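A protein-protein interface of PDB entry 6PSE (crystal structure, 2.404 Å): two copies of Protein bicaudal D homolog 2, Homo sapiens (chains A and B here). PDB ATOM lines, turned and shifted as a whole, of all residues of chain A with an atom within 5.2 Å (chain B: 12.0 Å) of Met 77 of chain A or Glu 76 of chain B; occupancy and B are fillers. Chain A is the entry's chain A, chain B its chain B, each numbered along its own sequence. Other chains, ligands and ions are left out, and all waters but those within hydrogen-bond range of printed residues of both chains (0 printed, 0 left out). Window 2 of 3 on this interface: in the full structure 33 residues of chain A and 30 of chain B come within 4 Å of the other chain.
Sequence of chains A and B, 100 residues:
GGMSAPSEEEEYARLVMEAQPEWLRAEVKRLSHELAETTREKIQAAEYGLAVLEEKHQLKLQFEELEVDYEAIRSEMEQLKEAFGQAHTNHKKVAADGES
The guanidinium group (NH2) of Arg 74 of chain A is in salt-bridge range of the side-chain carboxylate (OE2) of Glu 78 of chain A, 2.7 Å away.
Hydrophobic or aromatic side chains of chain B within 4 Å of the printed part of chain A: Tyr 70, Ile 73, Met 77 and Leu 80.
Among the printed residues, 9 pairs touch across the chains.
Among the printed residues, no Asp or Glu carboxylate lies within 4 Å of a Lys or Arg side-chain nitrogen of the other chain.
Arg 74 of chain A touches Ile 73 of chain B, but with the chains exchanged Ile 73 of chain A does not touch Arg 74 of chain B (4.1 Å).
Glu 76 of chain A touches Met 77 of chain B, and with the chains exchanged Met 77 of chain A touches Glu 76 of chain B.
Leu 80 of chain A touches Met 77 of chain B, but with the chains exchanged Met 77 of chain A does not touch Leu 80 of chain B (4.8 Å).
Leu 80 of chain A touches its own counterpart, Leu 80 of chain B.
9 positions are printed for both chains.
The side-chain sulfur (SD) of Met 77 of chain A lies close to the side-chain carboxylate (OE2) of Glu 76 of chain B, at 3.4 Å.
Among the printed residues, pairs that only touch across the chains: Ile 73 of chain A with Tyr 70 of chain B, Ile 73 of chain A with Ile 73 of chain B, Arg 74 of chain A with Ile 73 of chain B, Glu 76 of chain A with Met 77 of chain B, Met 77 of chain A with Ile 73 of chain B, Met 77 of chain A with Met 77 of chain B, Leu 80 of chain A with Met 77 of chain B and Leu 80 of chain A with Leu 80 of chain B.
Of the printed residues of chain B, Met 77 of chain A touches Ile 73, Glu 76 and Met 77.
Printed residues of chain A within 4 Å of Glu 76 of chain B: Met 77 (3.2 Å).
Of chain B, only Met 77 (3.6 Å) comes within 4 Å of Glu 76 of chain A.
Glu 78 of chain A touches none of the printed residues of chain B.
No residue of chain B comes within 4 Å of Gln 79 of chain A.
Printed residues of chain A within 4 Å of Ile 73 of chain B: Ile 73, Arg 74 and Met 77.
Of the printed residues of chain A, Tyr 70 of chain B touches Ile 73.
Of the printed residues of chain B, Arg 74 of chain A touches Ile 73.
Of the printed residues of chain A, Met 77 of chain B touches Glu 76 (3.6 Å), Met 77 (3.2 Å) and Leu 80 (3.4 Å).
The nearest printed residue of chain B that does not touch Arg 74 of chain A is Met 77 of chain B (6.2 Å).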
ATOM      1  N   ILE A  73      -8.417  21.719   3.853  1.00  0.00           N
ATOM      2  CA  ILE A  73      -8.551  22.547   5.046  1.00  0.00           C
ATOM      3  C   ILE A  73      -9.403  21.843   6.098  1.00  0.00           C
ATOM      4  O   ILE A  73      -9.025  21.750   7.267  1.00  0.00           O
ATOM      5  CB  ILE A  73      -9.153  23.914   4.690  1.00  0.00           C
ATOM      6  CG1 ILE A  73      -8.233  24.698   3.773  1.00  0.00           C
ATOM      7  CG2 ILE A  73      -9.422  24.717   5.961  1.00  0.00           C
ATOM      8  CD1 ILE A  73      -8.647  26.147   3.680  1.00  0.00           C
ATOM      9  N   ARG A  74     -10.579  21.369   5.699  1.00  0.00           N
ATOM     10  CA  ARG A  74     -11.483  20.733   6.652  1.00  0.00           C
ATOM     11  C   ARG A  74     -10.838  19.510   7.295  1.00  0.00           C
ATOM     12  O   ARG A  74     -10.973  19.284   8.503  1.00  0.00           O
ATOM     13  CB  ARG A  74     -12.770  20.355   5.932  1.00  0.00           C
ATOM     14  CG  ARG A  74     -13.981  20.224   6.799  1.00  0.00           C
ATOM     15  CD  ARG A  74     -14.681  18.940   6.449  1.00  0.00           C
ATOM     16  NE  ARG A  74     -13.760  17.836   6.669  1.00  0.00           N
ATOM     17  CZ  ARG A  74     -13.948  16.597   6.232  1.00  0.00           C
ATOM     18  NH1 ARG A  74     -15.041  16.287   5.540  1.00  0.00           N
ATOM     19  NH2 ARG A  74     -13.035  15.668   6.493  1.00  0.00           N
ATOM     20  N   SER A  75     -10.145  18.698   6.495  1.00  0.00           N
ATOM     21  CA  SER A  75      -9.389  17.579   7.035  1.00  0.00           C
ATOM     22  C   SER A  75      -8.440  18.025   8.138  1.00  0.00           C
ATOM     23  O   SER A  75      -8.331  17.360   9.178  1.00  0.00           O
ATOM     24  CB  SER A  75      -8.600  16.914   5.911  1.00  0.00           C
ATOM     25  OG  SER A  75      -7.978  15.718   6.354  1.00  0.00           O
ATOM     26  N   GLU A  76      -7.724  19.135   7.915  1.00  0.00           N
ATOM     27  CA  GLU A  76      -6.743  19.600   8.892  1.00  0.00           C
ATOM     28  C   GLU A  76      -7.417  20.053  10.180  1.00  0.00           C
ATOM     29  O   GLU A  76      -6.942  19.738  11.281  1.00  0.00           O
ATOM     30  CB  GLU A  76      -5.906  20.734   8.302  1.00  0.00           C
ATOM     31  CG  GLU A  76      -4.465  20.747   8.813  1.00  0.00           C
ATOM     32  CD  GLU A  76      -3.682  21.972   8.375  1.00  0.00           C
ATOM     33  OE1 GLU A  76      -3.606  22.255   7.155  1.00  0.00           O
ATOM     34  OE2 GLU A  76      -3.132  22.648   9.265  1.00  0.00           O
ATOM     35  N   MET A  77      -8.529  20.781  10.062  1.00  0.00           N
ATOM     36  CA  MET A  77      -9.269  21.297  11.212  1.00  0.00           C
ATOM     37  C   MET A  77      -9.767  20.209  12.129  1.00  0.00           C
ATOM     38  O   MET A  77      -9.535  20.260  13.331  1.00  0.00           O
ATOM     39  CB  MET A  77     -10.438  22.140  10.740  1.00  0.00           C
ATOM     40  CG  MET A  77     -11.172  22.808  11.861  1.00  0.00           C
ATOM     41  SD  MET A  77     -11.914  24.492  11.282  1.00  0.00           S
ATOM     42  CE  MET A  77     -13.491  23.800  10.342  1.00  0.00           C
ATOM     43  N   GLU A  78     -10.458  19.229  11.544  1.00  0.00           N
ATOM     44  CA  GLU A  78     -10.855  18.036  12.284  1.00  0.00           C
ATOM     45  C   GLU A  78      -9.694  17.455  13.081  1.00  0.00           C
ATOM     46  O   GLU A  78      -9.833  17.136  14.265  1.00  0.00           O
ATOM     47  CB  GLU A  78     -11.389  16.988  11.319  1.00  0.00           C
ATOM     48  CG  GLU A  78     -12.867  16.760  11.391  1.00  0.00           C
ATOM     49  CD  GLU A  78     -13.284  15.692  10.415  1.00  0.00           C
ATOM     50  OE1 GLU A  78     -13.822  14.653  10.862  1.00  0.00           O
ATOM     51  OE2 GLU A  78     -13.029  15.882   9.203  1.00  0.00           O
ATOM     52  N   GLN A  79      -8.541  17.292  12.437  1.00  0.00           N
ATOM     53  CA  GLN A  79      -7.378  16.788  13.147  1.00  0.00           C
ATOM     54  C   GLN A  79      -7.020  17.681  14.332  1.00  0.00           C
ATOM     55  O   GLN A  79      -6.582  17.183  15.377  1.00  0.00           O
ATOM     56  CB  GLN A  79      -6.202  16.668  12.174  1.00  0.00           C
ATOM     57  CG  GLN A  79      -4.833  17.027  12.771  1.00  0.00           C
ATOM     58  CD  GLN A  79      -4.308  15.951  13.702  1.00  0.00           C
ATOM     59  OE1 GLN A  79      -4.901  14.872  13.815  1.00  0.00           O
ATOM     60  NE2 GLN A  79      -3.173  16.222  14.354  1.00  0.00           N
ATOM     61  N   LEU A  80      -7.220  18.995  14.192  1.00  0.00           N
ATOM     62  CA  LEU A  80      -6.794  19.954  15.203  1.00  0.00           C
ATOM     63  C   LEU A  80      -7.665  19.941  16.448  1.00  0.00           C
ATOM     64  O   LEU A  80      -7.186  20.310  17.527  1.00  0.00           O
ATOM     65  CB  LEU A  80      -6.777  21.367  14.617  1.00  0.00           C
ATOM     66  CG  LEU A  80      -5.445  21.766  13.990  1.00  0.00           C
ATOM     67  CD1 LEU A  80      -5.419  23.257  13.715  1.00  0.00           C
ATOM     68  CD2 LEU A  80      -4.309  21.367  14.917  1.00  0.00           C
ATOM     69  N   LYS A  81      -8.927  19.531  16.325  1.00  0.00           N
ATOM     70  CA  LYS A  81      -9.843  19.503  17.453  1.00  0.00           C
ATOM     71  C   LYS A  81      -9.574  18.337  18.400  1.00  0.00           C
ATOM     72  O   LYS A  81     -10.494  17.888  19.099  1.00  0.00           O
ATOM     73  CB  LYS A  81     -11.282  19.471  16.947  1.00  0.00           C
ATOM     74  CG  LYS A  81     -11.538  20.472  15.848  1.00  0.00           C
ATOM     75  CD  LYS A  81     -11.164  21.879  16.289  1.00  0.00           C
ATOM     76  CE  LYS A  81     -11.809  22.928  15.395  1.00  0.00           C
ATOM     77  NZ  LYS A  81     -13.155  22.524  14.878  1.00  0.00           N
ATOM     78  N   LEU B  66     -20.101  27.153  -2.271  1.00  0.00           N
ATOM     79  CA  LEU B  66     -18.878  26.516  -1.790  1.00  0.00           C
ATOM     80  C   LEU B  66     -17.786  27.540  -1.510  1.00  0.00           C
ATOM     81  O   LEU B  66     -17.008  27.384  -0.560  1.00  0.00           O
ATOM     82  CB  LEU B  66     -18.394  25.493  -2.816  1.00  0.00           C
ATOM     83  CG  LEU B  66     -17.040  24.821  -2.603  1.00  0.00           C
ATOM     84  CD1 LEU B  66     -17.008  24.135  -1.245  1.00  0.00           C
ATOM     85  CD2 LEU B  66     -16.750  23.834  -3.741  1.00  0.00           C
ATOM     86  N   GLU B  67     -17.689  28.581  -2.337  1.00  0.00           N
ATOM     87  CA  GLU B  67     -16.709  29.623  -2.073  1.00  0.00           C
ATOM     88  C   GLU B  67     -16.918  30.224  -0.692  1.00  0.00           C
ATOM     89  O   GLU B  67     -15.982  30.313   0.109  1.00  0.00           O
ATOM     90  CB  GLU B  67     -16.797  30.701  -3.140  1.00  0.00           C
ATOM     91  CG  GLU B  67     -15.659  30.655  -4.104  1.00  0.00           C
ATOM     92  CD  GLU B  67     -15.928  31.476  -5.336  1.00  0.00           C
ATOM     93  OE1 GLU B  67     -14.970  31.747  -6.087  1.00  0.00           O
ATOM     94  OE2 GLU B  67     -17.099  31.858  -5.550  1.00  0.00           O
ATOM     95  N   VAL B  68     -18.157  30.629  -0.400  1.00  0.00           N
ATOM     96  CA  VAL B  68     -18.508  31.188   0.904  1.00  0.00           C
ATOM     97  C   VAL B  68     -18.118  30.231   2.026  1.00  0.00           C
ATOM     98  O   VAL B  68     -17.410  30.604   2.974  1.00  0.00           O
ATOM     99  CB  VAL B  68     -20.014  31.510   0.939  1.00  0.00           C
ATOM    100  CG1 VAL B  68     -20.517  31.600   2.378  1.00  0.00           C
ATOM    101  CG2 VAL B  68     -20.310  32.782   0.145  1.00  0.00           C
ATOM    102  N   ASP B  69     -18.582  28.982   1.942  1.00  0.00           N
ATOM    103  CA  ASP B  69     -18.256  28.000   2.969  1.00  0.00           C
ATOM    104  C   ASP B  69     -16.751  27.794   3.066  1.00  0.00           C
ATOM    105  O   ASP B  69     -16.213  27.622   4.171  1.00  0.00           O
ATOM    106  CB  ASP B  69     -18.975  26.686   2.681  1.00  0.00           C
ATOM    107  CG  ASP B  69     -20.490  26.866   2.557  1.00  0.00           C
ATOM    108  OD1 ASP B  69     -20.976  28.022   2.654  1.00  0.00           O
ATOM    109  OD2 ASP B  69     -21.194  25.852   2.345  1.00  0.00           O
ATOM    110  N   TYR B  70     -16.057  27.834   1.921  1.00  0.00           N
ATOM    111  CA  TYR B  70     -14.597  27.751   1.913  1.00  0.00           C
ATOM    112  C   TYR B  70     -13.974  28.889   2.717  1.00  0.00           C
ATOM    113  O   TYR B  70     -13.064  28.672   3.530  1.00  0.00           O
ATOM    114  CB  TYR B  70     -14.068  27.778   0.477  1.00  0.00           C
ATOM    115  CG  TYR B  70     -12.569  27.636   0.434  1.00  0.00           C
ATOM    116  CD1 TYR B  70     -11.973  26.391   0.577  1.00  0.00           C
ATOM    117  CD2 TYR B  70     -11.742  28.746   0.297  1.00  0.00           C
ATOM    118  CE1 TYR B  70     -10.591  26.243   0.570  1.00  0.00           C
ATOM    119  CE2 TYR B  70     -10.358  28.613   0.293  1.00  0.00           C
ATOM    120  CZ  TYR B  70      -9.786  27.354   0.429  1.00  0.00           C
ATOM    121  OH  TYR B  70      -8.408  27.188   0.428  1.00  0.00           O
ATOM    122  N   GLU B  71     -14.438  30.117   2.474  1.00  0.00           N
ATOM    123  CA  GLU B  71     -13.942  31.257   3.234  1.00  0.00           C
ATOM    124  C   GLU B  71     -14.304  31.128   4.701  1.00  0.00           C
ATOM    125  O   GLU B  71     -13.502  31.477   5.575  1.00  0.00           O
ATOM    126  CB  GLU B  71     -14.504  32.556   2.660  1.00  0.00           C
ATOM    127  CG  GLU B  71     -13.664  33.115   1.544  1.00  0.00           C
ATOM    128  CD  GLU B  71     -12.205  32.806   1.760  1.00  0.00           C
ATOM    129  OE1 GLU B  71     -11.632  32.094   0.907  1.00  0.00           O
ATOM    130  OE2 GLU B  71     -11.644  33.260   2.790  1.00  0.00           O
ATOM    131  N   ALA B  72     -15.510  30.623   4.981  1.00  0.00           N
ATOM    132  CA  ALA B  72     -15.951  30.430   6.358  1.00  0.00           C
ATOM    133  C   ALA B  72     -14.938  29.630   7.158  1.00  0.00           C
ATOM    134  O   ALA B  72     -14.593  30.011   8.281  1.00  0.00           O
ATOM    135  CB  ALA B  72     -17.307  29.727   6.387  1.00  0.00           C
ATOM    136  N   ILE B  73     -14.444  28.517   6.600  1.00  0.00           N
ATOM    137  CA  ILE B  73     -13.533  27.656   7.352  1.00  0.00           C
ATOM    138  C   ILE B  73     -12.074  27.930   7.044  1.00  0.00           C
ATOM    139  O   ILE B  73     -11.197  27.324   7.682  1.00  0.00           O
ATOM    140  CB  ILE B  73     -13.817  26.154   7.140  1.00  0.00           C
ATOM    141  CG1 ILE B  73     -13.306  25.691   5.787  1.00  0.00           C
ATOM    142  CG2 ILE B  73     -15.311  25.875   7.271  1.00  0.00           C
ATOM    143  CD1 ILE B  73     -13.289  24.194   5.671  1.00  0.00           C
ATOM    144  N   ARG B  74     -11.774  28.814   6.097  1.00  0.00           N
ATOM    145  CA  ARG B  74     -10.416  29.334   6.037  1.00  0.00           C
ATOM    146  C   ARG B  74     -10.212  30.376   7.131  1.00  0.00           C
ATOM    147  O   ARG B  74      -9.157  30.413   7.774  1.00  0.00           O
ATOM    148  CB  ARG B  74     -10.129  29.897   4.642  1.00  0.00           C
ATOM    149  CG  ARG B  74      -8.762  30.517   4.463  1.00  0.00           C
ATOM    150  CD  ARG B  74      -8.827  31.869   3.743  1.00  0.00           C
ATOM    151  NE  ARG B  74      -9.631  32.890   4.433  1.00  0.00           N
ATOM    152  CZ  ARG B  74      -9.382  33.385   5.650  1.00  0.00           C
ATOM    153  NH1 ARG B  74     -10.177  34.324   6.158  1.00  0.00           N
ATOM    154  NH2 ARG B  74      -8.347  32.957   6.366  1.00  0.00           N
ATOM    155  N   SER B  75     -11.241  31.193   7.393  1.00  0.00           N
ATOM    156  CA  SER B  75     -11.187  32.186   8.464  1.00  0.00           C
ATOM    157  C   SER B  75     -11.429  31.579   9.836  1.00  0.00           C
ATOM    158  O   SER B  75     -10.982  32.146  10.837  1.00  0.00           O
ATOM    159  CB  SER B  75     -12.230  33.278   8.245  1.00  0.00           C
ATOM    160  OG  SER B  75     -13.364  33.022   9.056  1.00  0.00           O
ATOM    161  N   GLU B  76     -12.164  30.467   9.914  1.00  0.00           N
ATOM    162  CA  GLU B  76     -12.396  29.820  11.199  1.00  0.00           C
ATOM    163  C   GLU B  76     -11.159  29.071  11.644  1.00  0.00           C
ATOM    164  O   GLU B  76     -10.871  28.998  12.844  1.00  0.00           O
ATOM    165  CB  GLU B  76     -13.599  28.876  11.132  1.00  0.00           C
ATOM    166  CG  GLU B  76     -13.832  28.076  12.419  1.00  0.00           C
ATOM    167  CD  GLU B  76     -14.489  26.720  12.174  1.00  0.00           C
ATOM    168  OE1 GLU B  76     -15.030  26.495  11.062  1.00  0.00           O
ATOM    169  OE2 GLU B  76     -14.450  25.871  13.097  1.00  0.00           O
ATOM    170  N   MET B  77     -10.413  28.509  10.703  1.00  0.00           N
ATOM    171  CA  MET B  77      -9.046  28.173  11.031  1.00  0.00           C
ATOM    172  C   MET B  77      -8.323  29.483  10.773  1.00  0.00           C
ATOM    173  O   MET B  77      -8.984  30.463  10.446  1.00  0.00           O
ATOM    174  CB  MET B  77      -8.495  27.016  10.210  1.00  0.00           C
ATOM    175  CG  MET B  77      -7.230  26.488  10.848  1.00  0.00           C
ATOM    176  SD  MET B  77      -6.330  25.118   9.876  1.00  0.00           S
ATOM    177  CE  MET B  77      -7.092  23.621  10.764  1.00  0.00           C
ATOM    178  N   GLU B  78      -6.998  29.532  10.929  1.00  0.00           N
ATOM    179  CA  GLU B  78      -6.296  30.811  10.968  1.00  0.00           C
ATOM    180  C   GLU B  78      -6.693  31.526  12.261  1.00  0.00           C
ATOM    181  O   GLU B  78      -5.819  31.949  13.019  1.00  0.00           O
ATOM    182  CB  GLU B  78      -6.590  31.649   9.709  1.00  0.00           C
ATOM    183  CG  GLU B  78      -6.491  33.147   9.882  1.00  0.00           C
ATOM    184  CD  GLU B  78      -5.068  33.636   9.756  1.00  0.00           C
ATOM    185  OE1 GLU B  78      -4.499  33.504   8.651  1.00  0.00           O
ATOM    186  OE2 GLU B  78      -4.517  34.133  10.765  1.00  0.00           O
ATOM    187  N   GLN B  79      -8.007  31.654  12.516  1.00  0.00           N
ATOM    188  CA  GLN B  79      -8.532  31.957  13.850  1.00  0.00           C
ATOM    189  C   GLN B  79      -7.943  31.026  14.898  1.00  0.00           C
ATOM    190  O   GLN B  79      -7.758  31.423  16.056  1.00  0.00           O
ATOM    191  CB  GLN B  79     -10.058  31.821  13.844  1.00  0.00           C
ATOM    192  CG  GLN B  79     -10.867  32.821  14.658  1.00  0.00           C
ATOM    193  CD  GLN B  79     -12.198  33.152  13.980  1.00  0.00           C
ATOM    194  OE1 GLN B  79     -13.133  32.344  13.989  1.00  0.00           O
ATOM    195  NE2 GLN B  79     -12.289  34.345  13.397  1.00  0.00           N
ATOM    196  N   LEU B  80      -7.665  29.778  14.522  1.00  0.00           N
ATOM    197  CA  LEU B  80      -6.864  28.887  15.350  1.00  0.00           C
ATOM    198  C   LEU B  80      -5.456  29.477  15.405  1.00  0.00           C
ATOM    199  O   LEU B  80      -4.640  29.257  14.507  1.00  0.00           O
ATOM    200  CB  LEU B  80      -6.892  27.462  14.787  1.00  0.00           C
ATOM    201  CG  LEU B  80      -8.282  26.804  14.602  1.00  0.00           C
ATOM    202  CD1 LEU B  80      -8.228  25.287  14.725  1.00  0.00           C
ATOM    203  CD2 LEU B  80      -9.296  27.357  15.589  1.00  0.00           C
ATOM    204  N   LYS B  81      -5.191  30.269  16.446  1.00  0.00           N
ATOM    205  CA  LYS B  81      -4.084  31.224  16.502  1.00  0.00           C
ATOM    206  C   LYS B  81      -3.418  31.139  17.864  1.00  0.00           C
ATOM    207  O   LYS B  81      -3.900  31.744  18.823  1.00  0.00           O
ATOM    208  CB  LYS B  81      -4.591  32.647  16.292  1.00  0.00           C
ATOM    209  CG  LYS B  81      -4.193  33.310  15.006  1.00  0.00           C
ATOM    210  CD  LYS B  81      -2.835  33.968  15.070  1.00  0.00           C
ATOM    211  CE  LYS B  81      -2.678  34.832  13.822  1.00  0.00           C
ATOM    212  NZ  LYS B  81      -1.293  34.808  13.268  1.00  0.00           N
ATOM    213  N   GLU B  82      -2.293  30.447  17.946  1.00  0.00           N
ATOM    214  CA  GLU B  82      -1.479  30.436  19.163  1.00  0.00           C
ATOM    215  C   GLU B  82       0.012  30.353  18.832  1.00  0.00           C
ATOM    216  O   GLU B  82       0.495  29.332  18.369  1.00  0.00           O
ATOM    217  CB  GLU B  82      -1.882  29.269  20.058  1.00  0.00           C
ATOM    218  CG  GLU B  82      -3.076  29.534  20.949  1.00  0.00           C
ATOM    219  CD  GLU B  82      -4.376  29.150  20.276  1.00  0.00           C
ATOM    220  OE1 GLU B  82      -4.392  28.074  19.651  1.00  0.00           O
ATOM    221  OE2 GLU B  82      -5.362  29.922  20.343  1.00  0.00           O
